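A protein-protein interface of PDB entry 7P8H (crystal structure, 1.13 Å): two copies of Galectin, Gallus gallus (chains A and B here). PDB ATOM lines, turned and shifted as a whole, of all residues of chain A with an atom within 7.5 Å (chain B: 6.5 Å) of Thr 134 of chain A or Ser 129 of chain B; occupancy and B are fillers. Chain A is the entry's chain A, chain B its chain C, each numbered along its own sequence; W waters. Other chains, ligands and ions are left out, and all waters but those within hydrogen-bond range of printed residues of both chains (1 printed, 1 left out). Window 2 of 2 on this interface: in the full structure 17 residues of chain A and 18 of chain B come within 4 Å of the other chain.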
ATOM      1  N   TYR A   9      -8.218  10.082  -4.942  1.00  0.00           N
ATOM      2  CA  TYR A   9      -7.574   8.794  -5.180  1.00  0.00           C
ATOM      3  C   TYR A   9      -8.311   7.799  -4.297  1.00  0.00           C
ATOM      4  O   TYR A   9      -7.975   7.646  -3.116  1.00  0.00           O
ATOM      5  CB  TYR A   9      -6.079   8.863  -4.870  1.00  0.00           C
ATOM      6  CG  TYR A   9      -5.373   7.557  -5.136  1.00  0.00           C
ATOM      7  CD1 TYR A   9      -5.074   7.160  -6.433  1.00  0.00           C
ATOM      8  CD2 TYR A   9      -5.025   6.707  -4.101  1.00  0.00           C
ATOM      9  CE1 TYR A   9      -4.443   5.957  -6.694  1.00  0.00           C
ATOM     10  CE2 TYR A   9      -4.389   5.490  -4.346  1.00  0.00           C
ATOM     11  CZ  TYR A   9      -4.103   5.132  -5.654  1.00  0.00           C
ATOM     12  OH  TYR A   9      -3.485   3.942  -5.919  1.00  0.00           O
ATOM     13  N   MET A  13      -4.620   7.686  -0.201  1.00  0.00           N
ATOM     14  CA  MET A  13      -3.305   8.260  -0.451  1.00  0.00           C
ATOM     15  C   MET A  13      -2.526   8.463   0.849  1.00  0.00           C
ATOM     16  O   MET A  13      -1.807   9.455   0.980  1.00  0.00           O
ATOM     17  CB  MET A  13      -3.403   9.560  -1.272  1.00  0.00           C
ATOM     18  CG  MET A  13      -4.202  10.744  -0.646  1.00  0.00           C
ATOM     19  SD  MET A  13      -4.123  12.345  -1.550  1.00  0.00           S
ATOM     20  CE  MET A  13      -5.071  11.954  -3.011  1.00  0.00           C
ATOM     21  N   GLY A  16       2.450   6.738   3.337  1.00  0.00           N
ATOM     22  CA  GLY A  16       3.447   6.370   2.349  1.00  0.00           C
ATOM     23  C   GLY A  16       3.296   7.060   1.015  1.00  0.00           C
ATOM     24  O   GLY A  16       3.729   6.515  -0.014  1.00  0.00           O
ATOM     25  N   TRP A  17       2.660   8.224   0.993  1.00  0.00           N
ATOM     26  CA  TRP A  17       2.577   9.044  -0.201  1.00  0.00           C
ATOM     27  C   TRP A  17       3.170  10.425   0.047  1.00  0.00           C
ATOM     28  O   TRP A  17       3.139  10.949   1.167  1.00  0.00           O
ATOM     29  CB  TRP A  17       1.112   9.235  -0.610  1.00  0.00           C
ATOM     30  CG  TRP A  17       0.459   8.006  -1.145  1.00  0.00           C
ATOM     31  CD1 TRP A  17       0.138   6.878  -0.458  1.00  0.00           C
ATOM     32  CD2 TRP A  17       0.037   7.789  -2.492  1.00  0.00           C
ATOM     33  NE1 TRP A  17      -0.457   5.961  -1.295  1.00  0.00           N
ATOM     34  CE2 TRP A  17      -0.534   6.500  -2.550  1.00  0.00           C
ATOM     35  CE3 TRP A  17       0.086   8.558  -3.656  1.00  0.00           C
ATOM     36  CZ2 TRP A  17      -1.053   5.968  -3.723  1.00  0.00           C
ATOM     37  CZ3 TRP A  17      -0.429   8.026  -4.818  1.00  0.00           C
ATOM     38  CH2 TRP A  17      -0.988   6.743  -4.842  1.00  0.00           C
ATOM     39  N   SER A  18       3.684  11.012  -1.027  1.00  0.00           N
ATOM     40  CA  SER A  18       4.157  12.382  -1.054  1.00  0.00           C
ATOM     41  C   SER A  18       3.235  13.220  -1.933  1.00  0.00           C
ATOM     42  O   SER A  18       2.845  12.794  -3.030  1.00  0.00           O
ATOM     43  CB  SER A  18       5.576  12.410  -1.641  1.00  0.00           C
ATOM     44  OG  SER A  18       5.952  13.678  -2.114  1.00  0.00           O
ATOM     45  N   VAL A  19       2.912  14.411  -1.459  1.00  0.00           N
ATOM     46  CA  VAL A  19       2.231  15.433  -2.242  1.00  0.00           C
ATOM     47  C   VAL A  19       3.168  16.634  -2.310  1.00  0.00           C
ATOM     48  O   VAL A  19       3.567  17.169  -1.267  1.00  0.00           O
ATOM     49  CB  VAL A  19       0.886  15.825  -1.613  1.00  0.00           C
ATOM     50  CG1 VAL A  19       0.254  16.988  -2.378  1.00  0.00           C
ATOM     51  CG2 VAL A  19      -0.043  14.642  -1.576  1.00  0.00           C
ATOM     52  N   VAL A  20       3.537  17.036  -3.522  1.00  0.00           N
ATOM     53  CA  VAL A  20       4.412  18.180  -3.727  1.00  0.00           C
ATOM     54  C   VAL A  20       3.606  19.244  -4.446  1.00  0.00           C
ATOM     55  O   VAL A  20       3.098  19.014  -5.548  1.00  0.00           O
ATOM     56  CB  VAL A  20       5.669  17.815  -4.533  1.00  0.00           C
ATOM     57  CG1 VAL A  20       6.542  19.040  -4.730  1.00  0.00           C
ATOM     58  CG2 VAL A  20       6.446  16.741  -3.815  1.00  0.00           C
ATOM     59  N   GLU A  87       6.253  20.075   0.260  1.00  0.00           N
ATOM     60  CA  GLU A  87       6.081  18.631   0.188  1.00  0.00           C
ATOM     61  C   GLU A  87       5.505  18.132   1.504  1.00  0.00           C
ATOM     62  O   GLU A  87       6.035  18.429   2.576  1.00  0.00           O
ATOM     63  CB  GLU A  87       7.389  17.903  -0.137  1.00  0.00           C
ATOM     64  CG  GLU A  87       7.221  16.376  -0.163  1.00  0.00           C
ATOM     65  CD  GLU A  87       8.361  15.651  -0.832  1.00  0.00           C
ATOM     66  OE1 GLU A  87       9.417  16.266  -1.060  1.00  0.00           O
ATOM     67  OE2 GLU A  87       8.206  14.447  -1.123  1.00  0.00           O
ATOM     68  N   ILE A  88       4.417  17.382   1.410  1.00  0.00           N
ATOM     69  CA  ILE A  88       3.799  16.725   2.548  1.00  0.00           C
ATOM     70  C   ILE A  88       3.938  15.224   2.323  1.00  0.00           C
ATOM     71  O   ILE A  88       3.383  14.679   1.364  1.00  0.00           O
ATOM     72  CB  ILE A  88       2.337  17.167   2.721  1.00  0.00           C
ATOM     73  CG1 ILE A  88       2.298  18.683   2.987  1.00  0.00           C
ATOM     74  CG2 ILE A  88       1.669  16.364   3.842  1.00  0.00           C
ATOM     75  CD1 ILE A  88       0.920  19.323   2.949  1.00  0.00           C
ATOM     76  N   TYR A  89       4.686  14.561   3.200  1.00  0.00           N
ATOM     77  CA  TYR A  89       4.912  13.122   3.128  1.00  0.00           C
ATOM     78  C   TYR A  89       4.354  12.481   4.384  1.00  0.00           C
ATOM     79  O   TYR A  89       4.683  12.913   5.484  1.00  0.00           O
ATOM     80  CB  TYR A  89       6.412  12.821   3.047  1.00  0.00           C
ATOM     81  CG  TYR A  89       6.707  11.353   3.208  1.00  0.00           C
ATOM     82  CD1 TYR A  89       6.356  10.453   2.222  1.00  0.00           C
ATOM     83  CD2 TYR A  89       7.294  10.852   4.368  1.00  0.00           C
ATOM     84  CE1 TYR A  89       6.593   9.099   2.373  1.00  0.00           C
ATOM     85  CE2 TYR A  89       7.540   9.489   4.525  1.00  0.00           C
ATOM     86  CZ  TYR A  89       7.184   8.628   3.520  1.00  0.00           C
ATOM     87  OH  TYR A  89       7.419   7.282   3.648  1.00  0.00           O
ATOM     88  N   GLU A 132       2.173  17.228  -7.588  1.00  0.00           N
ATOM     89  CA  GLU A 132       2.630  15.879  -7.856  1.00  0.00           C
ATOM     90  C   GLU A 132       2.291  14.997  -6.672  1.00  0.00           C
ATOM     91  O   GLU A 132       2.605  15.331  -5.531  1.00  0.00           O
ATOM     92  CB  GLU A 132       4.118  15.886  -8.101  1.00  0.00           C
ATOM     93  CG  GLU A 132       4.738  14.569  -8.406  1.00  0.00           C
ATOM     94  CD  GLU A 132       6.191  14.803  -8.599  1.00  0.00           C
ATOM     95  OE1 GLU A 132       6.559  15.202  -9.722  1.00  0.00           O
ATOM     96  OE2 GLU A 132       6.933  14.722  -7.601  1.00  0.00           O
ATOM     97  N   ILE A 133       1.645  13.882  -6.955  1.00  0.00           N
ATOM     98  CA  ILE A 133       1.187  12.944  -5.943  1.00  0.00           C
ATOM     99  C   ILE A 133       1.838  11.598  -6.250  1.00  0.00           C
ATOM    100  O   ILE A 133       1.610  11.033  -7.323  1.00  0.00           O
ATOM    101  CB  ILE A 133      -0.350  12.861  -5.967  1.00  0.00           C
ATOM    102  CG1 ILE A 133      -0.946  14.246  -5.670  1.00  0.00           C
ATOM    103  CG2 ILE A 133      -0.853  11.802  -5.013  1.00  0.00           C
ATOM    104  CD1 ILE A 133      -2.433  14.342  -5.868  1.00  0.00           C
ATOM    105  N   THR A 134       2.645  11.090  -5.321  1.00  0.00           N
ATOM    106  CA  THR A 134       3.530   9.961  -5.587  1.00  0.00           C
ATOM    107  C   THR A 134       3.466   8.950  -4.459  1.00  0.00           C
ATOM    108  O   THR A 134       3.598   9.302  -3.282  1.00  0.00           O
ATOM    109  CB  THR A 134       4.967  10.445  -5.730  1.00  0.00           C
ATOM    110  OG1 THR A 134       5.027  11.407  -6.777  1.00  0.00           O
ATOM    111  CG2 THR A 134       5.914   9.299  -6.060  1.00  0.00           C
ATOM    112  N   LYS A 135       3.277   7.699  -4.833  1.00  0.00           N
ATOM    113  CA  LYS A 135       3.306   6.590  -3.896  1.00  0.00           C
ATOM    114  C   LYS A 135       4.749   6.180  -3.621  1.00  0.00           C
ATOM    115  O   LYS A 135       5.636   6.322  -4.470  1.00  0.00           O
ATOM    116  CB  LYS A 135       2.583   5.394  -4.511  1.00  0.00           C
ATOM    117  CG  LYS A 135       2.374   4.249  -3.546  1.00  0.00           C
ATOM    118  CD  LYS A 135       2.256   2.943  -4.261  1.00  0.00           C
ATOM    119  CE  LYS A 135       0.984   2.893  -5.073  1.00  0.00           C
ATOM    120  NZ  LYS A 135       0.848   1.580  -5.778  1.00  0.00           N
ATOM    121  N   ARG A 136       4.989   5.644  -2.436  1.00  0.00           N
ATOM    122  CA  ARG A 136       6.364   5.494  -2.013  1.00  0.00           C
ATOM    123  C   ARG A 136       7.021   6.863  -2.149  1.00  0.00           C
ATOM    124  O   ARG A 136       7.824   7.135  -3.041  1.00  0.00           O
ATOM    125  CB  ARG A 136       7.080   4.439  -2.860  1.00  0.00           C
ATOM    126  CG  ARG A 136       6.279   3.157  -3.079  1.00  0.00           C
ATOM    127  CD  ARG A 136       7.171   2.063  -3.608  1.00  0.00           C
ATOM    128  NE  ARG A 136       8.335   1.911  -2.747  1.00  0.00           N
ATOM    129  CZ  ARG A 136       9.437   1.262  -3.083  1.00  0.00           C
ATOM    130  NH1 ARG A 136       9.554   0.664  -4.259  1.00  0.00           N
ATOM    131  NH2 ARG A 136      10.449   1.215  -2.218  1.00  0.00           N
ATOM    132  N   GLY A 137       6.543   7.750  -1.289  1.00  0.00           N
ATOM    133  CA  GLY A 137       6.893   9.148  -1.345  1.00  0.00           C
ATOM    134  C   GLY A 137       8.335   9.446  -1.047  1.00  0.00           C
ATOM    135  O   GLY A 137       8.736  10.612  -1.102  1.00  0.00           O
ATOM    136  N   LEU A 138       9.122   8.424  -0.709  1.00  0.00           N
ATOM    137  CA  LEU A 138      10.558   8.583  -0.554  1.00  0.00           C
ATOM    138  C   LEU A 138      11.284   8.662  -1.889  1.00  0.00           C
ATOM    139  O   LEU A 138      12.475   8.986  -1.904  1.00  0.00           O
ATOM    140  CB  LEU A 138      11.114   7.411   0.257  1.00  0.00           C
ATOM    141  CG  LEU A 138      10.543   7.230   1.665  1.00  0.00           C
ATOM    142  CD1 LEU A 138      11.101   5.957   2.301  1.00  0.00           C
ATOM    143  CD2 LEU A 138      10.846   8.450   2.528  1.00  0.00           C
ATOM    144  N   TYR A 139      10.601   8.392  -3.001  1.00  0.00           N
ATOM    145  CA  TYR A 139      11.248   8.302  -4.309  1.00  0.00           C
ATOM    146  C   TYR A 139      10.423   8.983  -5.401  1.00  0.00           C
ATOM    147  O   TYR A 139       9.661   9.915  -5.137  1.00  0.00           O
ATOM    148  CB  TYR A 139      11.472   6.831  -4.679  1.00  0.00           C
ATOM    149  CG  TYR A 139      12.125   6.028  -3.577  1.00  0.00           C
ATOM    150  CD1 TYR A 139      13.507   6.013  -3.424  1.00  0.00           C
ATOM    151  CD2 TYR A 139      11.358   5.293  -2.679  1.00  0.00           C
ATOM    152  CE1 TYR A 139      14.107   5.284  -2.408  1.00  0.00           C
ATOM    153  CE2 TYR A 139      11.947   4.561  -1.663  1.00  0.00           C
ATOM    154  CZ  TYR A 139      13.320   4.561  -1.532  1.00  0.00           C
ATOM    155  OH  TYR A 139      13.909   3.837  -0.523  1.00  0.00           O
ATOM    156  N   VAL B  21       1.724  10.590 -15.863  1.00  0.00           N
ATOM    157  CA  VAL B  21       1.167   9.464 -15.127  1.00  0.00           C
ATOM    158  C   VAL B  21       2.172   8.332 -15.202  1.00  0.00           C
ATOM    159  O   VAL B  21       2.583   7.935 -16.299  1.00  0.00           O
ATOM    160  CB  VAL B  21      -0.180   9.016 -15.719  1.00  0.00           C
ATOM    161  CG1 VAL B  21      -0.729   7.817 -14.936  1.00  0.00           C
ATOM    162  CG2 VAL B  21      -1.172  10.160 -15.728  1.00  0.00           C
ATOM    163  N   LYS B  22       2.575   7.832 -14.049  1.00  0.00           N
ATOM    164  CA  LYS B  22       3.407   6.646 -13.969  1.00  0.00           C
ATOM    165  C   LYS B  22       2.599   5.531 -13.337  1.00  0.00           C
ATOM    166  O   LYS B  22       1.856   5.748 -12.375  1.00  0.00           O
ATOM    167  CB  LYS B  22       4.677   6.919 -13.172  1.00  0.00           C
ATOM    168  CG  LYS B  22       5.520   7.987 -13.841  1.00  0.00           C
ATOM    169  CD  LYS B  22       6.685   8.436 -12.996  1.00  0.00           C
ATOM    170  CE  LYS B  22       7.776   7.418 -12.933  1.00  0.00           C
ATOM    171  NZ  LYS B  22       8.958   8.009 -12.229  1.00  0.00           N
ATOM    172  N   GLY B  23       2.747   4.332 -13.876  1.00  0.00           N
ATOM    173  CA  GLY B  23       2.071   3.182 -13.321  1.00  0.00           C
ATOM    174  C   GLY B  23       2.277   1.974 -14.209  1.00  0.00           C
ATOM    175  O   GLY B  23       3.143   1.967 -15.077  1.00  0.00           O
ATOM    176  N   LYS B  24       1.468   0.950 -13.970  1.00  0.00           N
ATOM    177  CA  LYS B  24       1.512  -0.269 -14.762  1.00  0.00           C
ATOM    178  C   LYS B  24       0.133  -0.911 -14.717  1.00  0.00           C
ATOM    179  O   LYS B  24      -0.653  -0.663 -13.800  1.00  0.00           O
ATOM    180  CB  LYS B  24       2.586  -1.244 -14.257  1.00  0.00           C
ATOM    181  CG  LYS B  24       2.332  -1.852 -12.895  1.00  0.00           C
ATOM    182  CD  LYS B  24       3.491  -2.770 -12.532  1.00  0.00           C
ATOM    183  CE  LYS B  24       3.381  -3.360 -11.143  1.00  0.00           C
ATOM    184  NZ  LYS B  24       4.411  -4.416 -10.923  1.00  0.00           N
ATOM    185  N   PHE B  84       5.332   2.160 -16.904  1.00  0.00           N
ATOM    186  CA  PHE B  84       5.420   3.134 -17.971  1.00  0.00           C
ATOM    187  C   PHE B  84       5.285   4.527 -17.386  1.00  0.00           C
ATOM    188  O   PHE B  84       4.853   4.702 -16.244  1.00  0.00           O
ATOM    189  CB  PHE B  84       4.328   2.924 -19.021  1.00  0.00           C
ATOM    190  CG  PHE B  84       2.934   2.871 -18.461  1.00  0.00           C
ATOM    191  CD1 PHE B  84       2.291   4.024 -18.065  1.00  0.00           C
ATOM    192  CD2 PHE B  84       2.251   1.666 -18.370  1.00  0.00           C
ATOM    193  CE1 PHE B  84       1.006   3.978 -17.556  1.00  0.00           C
ATOM    194  CE2 PHE B  84       0.958   1.620 -17.886  1.00  0.00           C
ATOM    195  CZ  PHE B  84       0.335   2.785 -17.478  1.00  0.00           C
ATOM    196  N   ILE B 126      -5.126   0.427 -14.397  1.00  0.00           N
ATOM    197  CA  ILE B 126      -3.835   1.060 -14.181  1.00  0.00           C
ATOM    198  C   ILE B 126      -3.607   1.161 -12.684  1.00  0.00           C
ATOM    199  O   ILE B 126      -4.464   1.665 -11.952  1.00  0.00           O
ATOM    200  CB  ILE B 126      -3.716   2.431 -14.876  1.00  0.00           C
ATOM    201  CG1 ILE B 126      -2.350   3.056 -14.582  1.00  0.00           C
ATOM    202  CG2 ILE B 126      -4.880   3.377 -14.487  1.00  0.00           C
ATOM    203  CD1 ILE B 126      -2.088   4.362 -15.321  1.00  0.00           C
ATOM    204  N   GLU B 127      -2.464   0.637 -12.236  1.00  0.00           N
ATOM    205  CA  GLU B 127      -1.990   0.805 -10.863  1.00  0.00           C
ATOM    206  C   GLU B 127      -1.079   2.023 -10.871  1.00  0.00           C
ATOM    207  O   GLU B 127       0.046   1.965 -11.372  1.00  0.00           O
ATOM    208  CB  GLU B 127      -1.219  -0.428 -10.408  1.00  0.00           C
ATOM    209  CG  GLU B 127      -2.002  -1.710 -10.472  1.00  0.00           C
ATOM    210  CD  GLU B 127      -1.177  -2.908 -10.046  1.00  0.00           C
ATOM    211  OE1 GLU B 127      -0.015  -2.734  -9.615  1.00  0.00           O
ATOM    212  OE2 GLU B 127      -1.699  -4.030 -10.130  1.00  0.00           O
ATOM    213  N   ILE B 128      -1.585   3.148 -10.366  1.00  0.00           N
ATOM    214  CA  ILE B 128      -0.872   4.420 -10.421  1.00  0.00           C
ATOM    215  C   ILE B 128       0.229   4.442  -9.374  1.00  0.00           C
ATOM    216  O   ILE B 128       0.003   4.128  -8.200  1.00  0.00           O
ATOM    217  CB  ILE B 128      -1.861   5.576 -10.195  1.00  0.00           C
ATOM    218  CG1 ILE B 128      -2.832   5.645 -11.370  1.00  0.00           C
ATOM    219  CG2 ILE B 128      -1.126   6.891  -9.976  1.00  0.00           C
ATOM    220  CD1 ILE B 128      -3.997   6.590 -11.122  1.00  0.00           C
ATOM    221  N   SER B 129       1.427   4.856  -9.784  1.00  0.00           N
ATOM    222  CA  SER B 129       2.484   5.176  -8.839  1.00  0.00           C
ATOM    223  C   SER B 129       2.686   6.672  -8.663  1.00  0.00           C
ATOM    224  O   SER B 129       3.144   7.091  -7.596  1.00  0.00           O
ATOM    225  CB  SER B 129       3.800   4.513  -9.240  1.00  0.00           C
ATOM    226  OG  SER B 129       4.276   4.996 -10.469  1.00  0.00           O
ATOM    227  N   SER B 130       2.336   7.488  -9.657  1.00  0.00           N
ATOM    228  CA  SER B 130       2.402   8.926  -9.471  1.00  0.00           C
ATOM    229  C   SER B 130       1.598   9.627 -10.552  1.00  0.00           C
ATOM    230  O   SER B 130       1.436   9.133 -11.668  1.00  0.00           O
ATOM    231  CB  SER B 130       3.844   9.453  -9.435  1.00  0.00           C
ATOM    232  OG  SER B 130       4.527   9.204 -10.645  1.00  0.00           O
ATOM    233  N   VAL B 131       1.062  10.786 -10.175  1.00  0.00           N
ATOM    234  CA  VAL B 131       0.438  11.718 -11.104  1.00  0.00           C
ATOM    235  C   VAL B 131       1.002  13.101 -10.829  1.00  0.00           C
ATOM    236  O   VAL B 131       0.961  13.576  -9.689  1.00  0.00           O
ATOM    237  CB  VAL B 131      -1.098  11.755 -11.012  1.00  0.00           C
ATOM    238  CG1 VAL B 131      -1.668  12.698 -12.069  1.00  0.00           C
ATOM    239  CG2 VAL B 131      -1.690  10.369 -11.165  1.00  0.00           C
HETATM  240  O   HOH W   1      -1.528   2.248  -7.141  1.00  0.00           O
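The backbone NH (N) of Lys 22 of chain B is in hydrogen-bond range of the backbone carbonyl oxygen (O) of Ser 130 of chain B. O of Thr 134 of chain A sits at hydrogen-bond distance from N of Ser 18 of chain A, 2.8 Å away. The backbone NH (N) of Ser 129 of chain B sits at hydrogen-bond distance from the backbone carbonyl oxygen (O) of Lys 22 of chain B, at 2.8 Å. The backbone NH (N) of Val 20 of chain A sits at hydrogen-bond distance from the backbone carbonyl oxygen (O) of Glu 132 of chain A (2.8 Å).
Met 13 of chain A touches none of the printed residues of chain B. Ser 18 of chain A touches none of the printed residues of chain B. Printed residues of chain B within 4 Å of Thr 134 of chain A: Ser 129 and Ser 130. Of the printed residues of chain A, Ile 128 of chain B touches Lys 135. Of chain A, only Thr 134 and Lys 135 come within 4 Å of Ser 129 of chain B. Printed residues of chain A within 4 Å of Val 131 of chain B: Glu 132 (3.4 Å) and Ile 133 (2.8 Å). The nearest residue of chain A that does not touch Ser 129 of chain B is Ile 133 of chain A (4.2 Å). The nearest printed residue of chain B that does not touch Glu 132 of chain A is Ser 130 of chain B (5.3 Å).
The backbone NH of Lys 135 of chain A lies within hydrogen-bond range of the backbone carbonyl oxygen of Ser 129 of chain B, 2.8 Å away. N of Ile 133 of chain A is in hydrogen-bond range of O of Val 131 of chain B, 2.8 Å away.
Among the printed residues, pairs that only touch across the chains: Glu 132 of chain A with Val 131 of chain B (3.4 Å), Ile 133 of chain A with Ser 130 of chain B (3.1 Å), Thr 134 of chain A with Ser 129 of chain B (3.5 Å), Thr 134 of chain A with Ser 130 of chain B (3.5 Å) and Lys 135 of chain A with Ile 128 of chain B (3.5 Å).
No position is printed for both chains. Of the 7 pairs that touch across the chains among the printed residues, none has its exchanged pair printed and touching as well.
Water W1 lies within hydrogen-bond range of O of Ile 128 of chain B (2.6 Å), NZ of Lys 135 of chain A (2.8 Å) and OH of Tyr 9 of chain A (2.9 Å).
Along chain A the printed residues that touch a printed residue of chain B span positions 132 to 135. Among the printed residues, 7 pairs touch across the chains.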
